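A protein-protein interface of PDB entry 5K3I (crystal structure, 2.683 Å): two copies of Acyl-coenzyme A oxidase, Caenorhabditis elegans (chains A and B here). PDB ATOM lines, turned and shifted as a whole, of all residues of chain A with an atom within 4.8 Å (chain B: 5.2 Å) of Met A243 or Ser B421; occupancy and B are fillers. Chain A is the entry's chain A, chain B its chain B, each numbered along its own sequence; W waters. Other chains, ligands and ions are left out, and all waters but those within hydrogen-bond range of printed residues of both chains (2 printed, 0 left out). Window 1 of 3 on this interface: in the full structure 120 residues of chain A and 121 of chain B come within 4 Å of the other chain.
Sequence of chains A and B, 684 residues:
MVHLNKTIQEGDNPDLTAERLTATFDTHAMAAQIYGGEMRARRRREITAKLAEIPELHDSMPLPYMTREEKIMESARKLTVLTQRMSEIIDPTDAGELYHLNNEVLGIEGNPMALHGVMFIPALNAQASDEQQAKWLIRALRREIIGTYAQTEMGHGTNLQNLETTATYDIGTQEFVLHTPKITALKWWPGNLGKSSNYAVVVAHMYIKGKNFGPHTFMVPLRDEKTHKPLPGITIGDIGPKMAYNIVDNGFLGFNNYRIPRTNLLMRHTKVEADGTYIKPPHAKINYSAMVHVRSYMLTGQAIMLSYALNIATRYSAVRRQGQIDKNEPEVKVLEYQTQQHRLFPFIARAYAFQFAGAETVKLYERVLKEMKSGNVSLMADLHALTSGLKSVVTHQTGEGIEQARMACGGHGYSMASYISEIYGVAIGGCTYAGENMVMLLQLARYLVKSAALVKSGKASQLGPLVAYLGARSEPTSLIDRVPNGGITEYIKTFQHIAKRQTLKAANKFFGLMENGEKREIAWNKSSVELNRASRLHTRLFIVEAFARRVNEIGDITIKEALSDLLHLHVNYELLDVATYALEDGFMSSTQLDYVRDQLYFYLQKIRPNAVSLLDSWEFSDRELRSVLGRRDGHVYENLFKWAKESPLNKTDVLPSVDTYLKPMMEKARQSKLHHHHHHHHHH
Tyr B424 touches its own counterpart, Tyr A424. 2 positions are printed for both chains. Of the 14 pairs that touch across the chains among the printed residues, 1 has its exchanged pair printed and touching as well.
The side-chain sulfur (SD) of Met B416 lies within hydrogen-bond range of the side-chain hydroxyl (OG) of Ser B421 (3.3 Å). The guanidinium group (NE) of Arg B406 lies within salt-bridge range of the side-chain carboxylate (OE2) of Glu B403 (2.7 Å). The backbone NH (N) of Lys A242 is in hydrogen-bond range of the side-chain amide oxygen (OD1) of Asn A246 (2.9 Å). The backbone carbonyl oxygen (O) of Ser B415 lies within hydrogen-bond range of the side-chain hydroxyl (OG) of Ser B418 (3.2 Å).
Among the printed residues, pairs that only touch across the chains: Ala A244 with Tyr B414, Met A243 with Ser B421, Tyr A424 with Tyr B424, Ile A428 with Arg B406, Lys A242 with Tyr B414, Met A243 with Glu B403 and Pro A241 with Ser B415.
Water W1 lies within hydrogen-bond range of the side-chain hydroxyl (OG) of Ser B415 and the backbone carbonyl oxygen (O) of Pro A241. Water W2 bridges the backbone carbonyl oxygen (O) of Ile A428 and the guanidinium group (NH1) of Arg B406.
The backbone NH (N) of Met A243 sits at hydrogen-bond distance from the backbone carbonyl oxygen (O) of Tyr B414 (2.9 Å). The backbone NH of Met A243 sits at hydrogen-bond distance from the side-chain sulfur of Met B416, at 3.8 Å. O of Lys A242 sits close to SD of Met B416. O of Pro A241 is in hydrogen-bond range of N of Met B416 (3.2 Å). The side-chain carboxylate (OE1) of Glu B403 is in hydrogen-bond range of the side-chain hydroxyl (OH) of Tyr A424 (2.5 Å). SD of Met A243 is in hydrogen-bond range of NE of Arg B406. The backbone carbonyl oxygen (O) of Gly A425 sits at hydrogen-bond distance from the side-chain hydroxyl (OH) of Tyr B414.
Of the 8 printed residues of chain A, 7 touch a printed residue of chain B. Hydrophobic or aromatic side chains of chain A that line the printed part of chain B: Met A243, Ala A244, Tyr A424 and Ile A428. Of the 14 printed residues of chain B, 7 touch a printed residue of chain A. Among the printed residues, no Asp or Glu carboxylate lies within 4 Å of a Lys or Arg side-chain nitrogen of the other chain.
Printed residues of chain B within 4 Å of Lys A242: Tyr B414 (3.6 Å) and Met B416 (3.5 Å). Of the printed residues of chain A, Glu B403 touches Met A243 (3.9 Å) and Tyr A424 (2.5 Å). Of chain A, only Met A243 comes within 4 Å of Ser B421. The nearest residue of chain B that does not touch Met A243 is Ser B415 (4.8 Å).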
ATOM      1  N   PRO A 241       9.903 -36.173 -14.942  1.00  0.00           N
ATOM      2  CA  PRO A 241      10.549 -35.582 -16.116  1.00  0.00           C
ATOM      3  C   PRO A 241      11.496 -34.457 -15.719  1.00  0.00           C
ATOM      4  O   PRO A 241      11.491 -33.951 -14.599  1.00  0.00           O
ATOM      5  CB  PRO A 241       9.375 -35.056 -16.949  1.00  0.00           C
ATOM      6  CG  PRO A 241       8.338 -34.727 -15.936  1.00  0.00           C
ATOM      7  CD  PRO A 241       8.493 -35.757 -14.832  1.00  0.00           C
ATOM      8  N   LYS A 242      12.316 -34.059 -16.686  1.00  0.00           N
ATOM      9  CA  LYS A 242      13.454 -33.202 -16.395  1.00  0.00           C
ATOM     10  C   LYS A 242      13.632 -32.203 -17.521  1.00  0.00           C
ATOM     11  O   LYS A 242      12.956 -32.261 -18.556  1.00  0.00           O
ATOM     12  CB  LYS A 242      14.749 -34.009 -16.236  1.00  0.00           C
ATOM     13  CG  LYS A 242      14.739 -35.000 -15.104  1.00  0.00           C
ATOM     14  CD  LYS A 242      15.981 -35.870 -15.109  1.00  0.00           C
ATOM     15  CE  LYS A 242      16.152 -36.483 -16.470  1.00  0.00           C
ATOM     16  NZ  LYS A 242      16.217 -37.957 -16.430  1.00  0.00           N
ATOM     17  N   MET A 243      14.577 -31.287 -17.292  1.00  0.00           N
ATOM     18  CA  MET A 243      14.960 -30.295 -18.287  1.00  0.00           C
ATOM     19  C   MET A 243      15.313 -30.951 -19.617  1.00  0.00           C
ATOM     20  O   MET A 243      14.909 -30.479 -20.686  1.00  0.00           O
ATOM     21  CB  MET A 243      16.129 -29.476 -17.746  1.00  0.00           C
ATOM     22  CG  MET A 243      16.860 -28.667 -18.757  1.00  0.00           C
ATOM     23  SD  MET A 243      18.009 -27.612 -17.890  1.00  0.00           S
ATOM     24  CE  MET A 243      18.101 -26.211 -18.989  1.00  0.00           C
ATOM     25  N   ALA A 244      16.071 -32.037 -19.567  1.00  0.00           N
ATOM     26  CA  ALA A 244      16.462 -32.807 -20.739  1.00  0.00           C
ATOM     27  C   ALA A 244      16.943 -34.162 -20.232  1.00  0.00           C
ATOM     28  O   ALA A 244      16.717 -34.518 -19.070  1.00  0.00           O
ATOM     29  CB  ALA A 244      17.532 -32.078 -21.561  1.00  0.00           C
ATOM     30  N   ASN A 246      15.904 -37.157 -20.833  1.00  0.00           N
ATOM     31  CA  ASN A 246      14.718 -37.814 -20.299  1.00  0.00           C
ATOM     32  C   ASN A 246      14.639 -39.308 -20.609  1.00  0.00           C
ATOM     33  O   ASN A 246      13.712 -39.966 -20.124  1.00  0.00           O
ATOM     34  CB  ASN A 246      13.478 -37.076 -20.794  1.00  0.00           C
ATOM     35  CG  ASN A 246      13.185 -35.836 -19.963  1.00  0.00           C
ATOM     36  OD1 ASN A 246      12.871 -35.935 -18.778  1.00  0.00           O
ATOM     37  ND2 ASN A 246      13.335 -34.662 -20.567  1.00  0.00           N
ATOM     38  N   TYR A 424      21.795 -28.583 -25.680  1.00  0.00           N
ATOM     39  CA  TYR A 424      22.020 -27.638 -24.587  1.00  0.00           C
ATOM     40  C   TYR A 424      21.581 -28.157 -23.217  1.00  0.00           C
ATOM     41  O   TYR A 424      22.323 -28.050 -22.240  1.00  0.00           O
ATOM     42  CB  TYR A 424      21.327 -26.306 -24.886  1.00  0.00           C
ATOM     43  CG  TYR A 424      21.434 -25.297 -23.765  1.00  0.00           C
ATOM     44  CD1 TYR A 424      22.612 -24.595 -23.546  1.00  0.00           C
ATOM     45  CD2 TYR A 424      20.356 -25.045 -22.926  1.00  0.00           C
ATOM     46  CE1 TYR A 424      22.714 -23.670 -22.524  1.00  0.00           C
ATOM     47  CE2 TYR A 424      20.448 -24.123 -21.901  1.00  0.00           C
ATOM     48  CZ  TYR A 424      21.629 -23.439 -21.704  1.00  0.00           C
ATOM     49  OH  TYR A 424      21.726 -22.520 -20.685  1.00  0.00           O
ATOM     50  N   GLY A 425      20.376 -28.711 -23.148  1.00  0.00           N
ATOM     51  CA  GLY A 425      19.839 -29.222 -21.896  1.00  0.00           C
ATOM     52  C   GLY A 425      20.654 -30.368 -21.338  1.00  0.00           C
ATOM     53  O   GLY A 425      20.830 -30.485 -20.124  1.00  0.00           O
ATOM     54  N   ILE A 428      24.426 -29.004 -20.307  1.00  0.00           N
ATOM     55  CA  ILE A 428      24.483 -28.076 -19.183  1.00  0.00           C
ATOM     56  C   ILE A 428      24.334 -28.814 -17.859  1.00  0.00           C
ATOM     57  O   ILE A 428      24.806 -28.337 -16.815  1.00  0.00           O
ATOM     58  CB  ILE A 428      23.417 -26.983 -19.357  1.00  0.00           C
ATOM     59  CG1 ILE A 428      23.798 -25.745 -18.546  1.00  0.00           C
ATOM     60  CG2 ILE A 428      22.053 -27.470 -18.910  1.00  0.00           C
ATOM     61  CD1 ILE A 428      24.859 -24.867 -19.234  1.00  0.00           C
ATOM     62  N   GLU B 403      19.256 -19.061 -15.635  1.00  0.00           N
ATOM     63  CA  GLU B 403      20.065 -20.277 -15.551  1.00  0.00           C
ATOM     64  C   GLU B 403      20.927 -20.328 -14.290  1.00  0.00           C
ATOM     65  O   GLU B 403      21.161 -21.419 -13.762  1.00  0.00           O
ATOM     66  CB  GLU B 403      20.919 -20.444 -16.800  1.00  0.00           C
ATOM     67  CG  GLU B 403      20.107 -21.004 -17.951  1.00  0.00           C
ATOM     68  CD  GLU B 403      19.886 -22.506 -17.863  1.00  0.00           C
ATOM     69  OE1 GLU B 403      20.616 -23.251 -18.555  1.00  0.00           O
ATOM     70  OE2 GLU B 403      18.977 -22.933 -17.110  1.00  0.00           O
ATOM     71  N   ARG B 406      18.388 -21.565 -11.695  1.00  0.00           N
ATOM     72  CA  ARG B 406      18.228 -23.017 -11.758  1.00  0.00           C
ATOM     73  C   ARG B 406      19.375 -23.743 -11.075  1.00  0.00           C
ATOM     74  O   ARG B 406      19.156 -24.623 -10.237  1.00  0.00           O
ATOM     75  CB  ARG B 406      18.134 -23.490 -13.202  1.00  0.00           C
ATOM     76  CG  ARG B 406      17.871 -24.984 -13.269  1.00  0.00           C
ATOM     77  CD  ARG B 406      17.653 -25.455 -14.679  1.00  0.00           C
ATOM     78  NE  ARG B 406      18.787 -25.101 -15.526  1.00  0.00           N
ATOM     79  CZ  ARG B 406      19.983 -25.681 -15.466  1.00  0.00           C
ATOM     80  NH1 ARG B 406      20.228 -26.638 -14.578  1.00  0.00           N
ATOM     81  NH2 ARG B 406      20.949 -25.285 -16.287  1.00  0.00           N
ATOM     82  N   GLY B 413      17.180 -28.510  -9.329  1.00  0.00           N
ATOM     83  CA  GLY B 413      16.864 -27.512 -10.335  1.00  0.00           C
ATOM     84  C   GLY B 413      16.682 -28.117 -11.711  1.00  0.00           C
ATOM     85  O   GLY B 413      15.882 -27.625 -12.516  1.00  0.00           O
ATOM     86  N   TYR B 414      17.411 -29.194 -11.997  1.00  0.00           N
ATOM     87  CA  TYR B 414      17.319 -29.844 -13.293  1.00  0.00           C
ATOM     88  C   TYR B 414      16.003 -30.583 -13.467  1.00  0.00           C
ATOM     89  O   TYR B 414      15.626 -30.896 -14.602  1.00  0.00           O
ATOM     90  CB  TYR B 414      18.497 -30.806 -13.458  1.00  0.00           C
ATOM     91  CG  TYR B 414      18.784 -31.218 -14.881  1.00  0.00           C
ATOM     92  CD1 TYR B 414      19.446 -30.368 -15.754  1.00  0.00           C
ATOM     93  CD2 TYR B 414      18.406 -32.464 -15.346  1.00  0.00           C
ATOM     94  CE1 TYR B 414      19.710 -30.745 -17.052  1.00  0.00           C
ATOM     95  CE2 TYR B 414      18.670 -32.852 -16.639  1.00  0.00           C
ATOM     96  CZ  TYR B 414      19.322 -31.986 -17.490  1.00  0.00           C
ATOM     97  OH  TYR B 414      19.598 -32.356 -18.786  1.00  0.00           O
ATOM     98  N   SER B 415      15.330 -30.906 -12.367  1.00  0.00           N
ATOM     99  CA  SER B 415      14.018 -31.524 -12.420  1.00  0.00           C
ATOM    100  C   SER B 415      12.969 -30.494 -12.813  1.00  0.00           C
ATOM    101  O   SER B 415      13.131 -29.294 -12.589  1.00  0.00           O
ATOM    102  CB  SER B 415      13.667 -32.144 -11.064  1.00  0.00           C
ATOM    103  OG  SER B 415      12.329 -32.605 -11.033  1.00  0.00           O
ATOM    104  N   MET B 416      11.882 -30.974 -13.421  1.00  0.00           N
ATOM    105  CA  MET B 416      10.780 -30.070 -13.726  1.00  0.00           C
ATOM    106  C   MET B 416      10.004 -29.691 -12.476  1.00  0.00           C
ATOM    107  O   MET B 416       9.122 -28.832 -12.546  1.00  0.00           O
ATOM    108  CB  MET B 416       9.816 -30.694 -14.740  1.00  0.00           C
ATOM    109  CG  MET B 416      10.427 -31.063 -16.083  1.00  0.00           C
ATOM    110  SD  MET B 416      11.189 -29.679 -16.953  1.00  0.00           S
ATOM    111  CE  MET B 416       9.872 -28.484 -17.003  1.00  0.00           C
ATOM    112  N   SER B 418      11.376 -28.028 -10.252  1.00  0.00           N
ATOM    113  CA  SER B 418      11.765 -26.629 -10.106  1.00  0.00           C
ATOM    114  C   SER B 418      10.969 -25.732 -11.045  1.00  0.00           C
ATOM    115  O   SER B 418      10.591 -24.618 -10.667  1.00  0.00           O
ATOM    116  CB  SER B 418      13.254 -26.461 -10.379  1.00  0.00           C
ATOM    117  OG  SER B 418      13.479 -26.254 -11.761  1.00  0.00           O
ATOM    118  N   TYR B 419      10.721 -26.204 -12.271  1.00  0.00           N
ATOM    119  CA  TYR B 419      10.103 -25.498 -13.395  1.00  0.00           C
ATOM    120  C   TYR B 419      10.983 -24.414 -14.008  1.00  0.00           C
ATOM    121  O   TYR B 419      10.567 -23.789 -14.995  1.00  0.00           O
ATOM    122  CB  TYR B 419       8.754 -24.880 -13.002  1.00  0.00           C
ATOM    123  CG  TYR B 419       7.788 -24.666 -14.146  1.00  0.00           C
ATOM    124  CD1 TYR B 419       7.341 -25.736 -14.915  1.00  0.00           C
ATOM    125  CD2 TYR B 419       7.280 -23.401 -14.423  1.00  0.00           C
ATOM    126  CE1 TYR B 419       6.439 -25.544 -15.948  1.00  0.00           C
ATOM    127  CE2 TYR B 419       6.382 -23.204 -15.444  1.00  0.00           C
ATOM    128  CZ  TYR B 419       5.963 -24.273 -16.205  1.00  0.00           C
ATOM    129  OH  TYR B 419       5.064 -24.050 -17.221  1.00  0.00           O
ATOM    130  N   ILE B 420      12.181 -24.170 -13.475  1.00  0.00           N
ATOM    131  CA  ILE B 420      12.995 -23.078 -14.002  1.00  0.00           C
ATOM    132  C   ILE B 420      13.459 -23.368 -15.430  1.00  0.00           C
ATOM    133  O   ILE B 420      13.649 -22.443 -16.227  1.00  0.00           O
ATOM    134  CB  ILE B 420      14.185 -22.787 -13.064  1.00  0.00           C
ATOM    135  CG1 ILE B 420      13.680 -22.340 -11.689  1.00  0.00           C
ATOM    136  CG2 ILE B 420      15.075 -21.725 -13.638  1.00  0.00           C
ATOM    137  CD1 ILE B 420      14.798 -22.066 -10.690  1.00  0.00           C
ATOM    138  N   SER B 421      13.648 -24.639 -15.786  1.00  0.00           N
ATOM    139  CA  SER B 421      14.117 -24.954 -17.133  1.00  0.00           C
ATOM    140  C   SER B 421      13.095 -24.547 -18.187  1.00  0.00           C
ATOM    141  O   SER B 421      13.468 -24.114 -19.280  1.00  0.00           O
ATOM    142  CB  SER B 421      14.456 -26.436 -17.254  1.00  0.00           C
ATOM    143  OG  SER B 421      13.287 -27.216 -17.426  1.00  0.00           O
ATOM    144  N   GLU B 422      11.801 -24.662 -17.877  1.00  0.00           N
ATOM    145  CA  GLU B 422      10.776 -24.211 -18.816  1.00  0.00           C
ATOM    146  C   GLU B 422      10.725 -22.688 -18.855  1.00  0.00           C
ATOM    147  O   GLU B 422      10.622 -22.093 -19.934  1.00  0.00           O
ATOM    148  CB  GLU B 422       9.406 -24.801 -18.437  1.00  0.00           C
ATOM    149  CG  GLU B 422       8.270 -24.501 -19.439  1.00  0.00           C
ATOM    150  CD  GLU B 422       8.467 -25.152 -20.798  1.00  0.00           C
ATOM    151  OE1 GLU B 422       9.066 -26.252 -20.859  1.00  0.00           O
ATOM    152  OE2 GLU B 422       7.992 -24.577 -21.798  1.00  0.00           O
ATOM    153  N   ILE B 423      10.760 -22.045 -17.682  1.00  0.00           N
ATOM    154  CA  ILE B 423      10.882 -20.587 -17.636  1.00  0.00           C
ATOM    155  C   ILE B 423      12.029 -20.132 -18.532  1.00  0.00           C
ATOM    156  O   ILE B 423      11.940 -19.101 -19.210  1.00  0.00           O
ATOM    157  CB  ILE B 423      11.078 -20.108 -16.180  1.00  0.00           C
ATOM    158  CG1 ILE B 423       9.829 -20.368 -15.340  1.00  0.00           C
ATOM    159  CG2 ILE B 423      11.427 -18.641 -16.132  1.00  0.00           C
ATOM    160  CD1 ILE B 423      10.063 -20.224 -13.858  1.00  0.00           C
ATOM    161  N   TYR B 424      13.120 -20.901 -18.559  1.00  0.00           N
ATOM    162  CA  TYR B 424      14.271 -20.500 -19.358  1.00  0.00           C
ATOM    163  C   TYR B 424      13.971 -20.625 -20.847  1.00  0.00           C
ATOM    164  O   TYR B 424      14.204 -19.687 -21.619  1.00  0.00           O
ATOM    165  CB  TYR B 424      15.505 -21.326 -18.988  1.00  0.00           C
ATOM    166  CG  TYR B 424      16.658 -21.024 -19.914  1.00  0.00           C
ATOM    167  CD1 TYR B 424      17.378 -19.842 -19.779  1.00  0.00           C
ATOM    168  CD2 TYR B 424      16.987 -21.885 -20.962  1.00  0.00           C
ATOM    169  CE1 TYR B 424      18.414 -19.541 -20.637  1.00  0.00           C
ATOM    170  CE2 TYR B 424      18.027 -21.587 -21.835  1.00  0.00           C
ATOM    171  CZ  TYR B 424      18.735 -20.414 -21.665  1.00  0.00           C
ATOM    172  OH  TYR B 424      19.768 -20.109 -22.522  1.00  0.00           O
ATOM    173  N   GLY B 425      13.471 -21.793 -21.267  1.00  0.00           N
ATOM    174  CA  GLY B 425      13.218 -22.030 -22.683  1.00  0.00           C
ATOM    175  C   GLY B 425      12.276 -21.016 -23.289  1.00  0.00           C
ATOM    176  O   GLY B 425      12.434 -20.625 -24.444  1.00  0.00           O
HETATM  177  O   HOH W   1      12.731 -34.735 -12.390  1.00  0.00           O
HETATM  178  O   HOH W   2      22.860 -27.556 -15.062  1.00  0.00           O
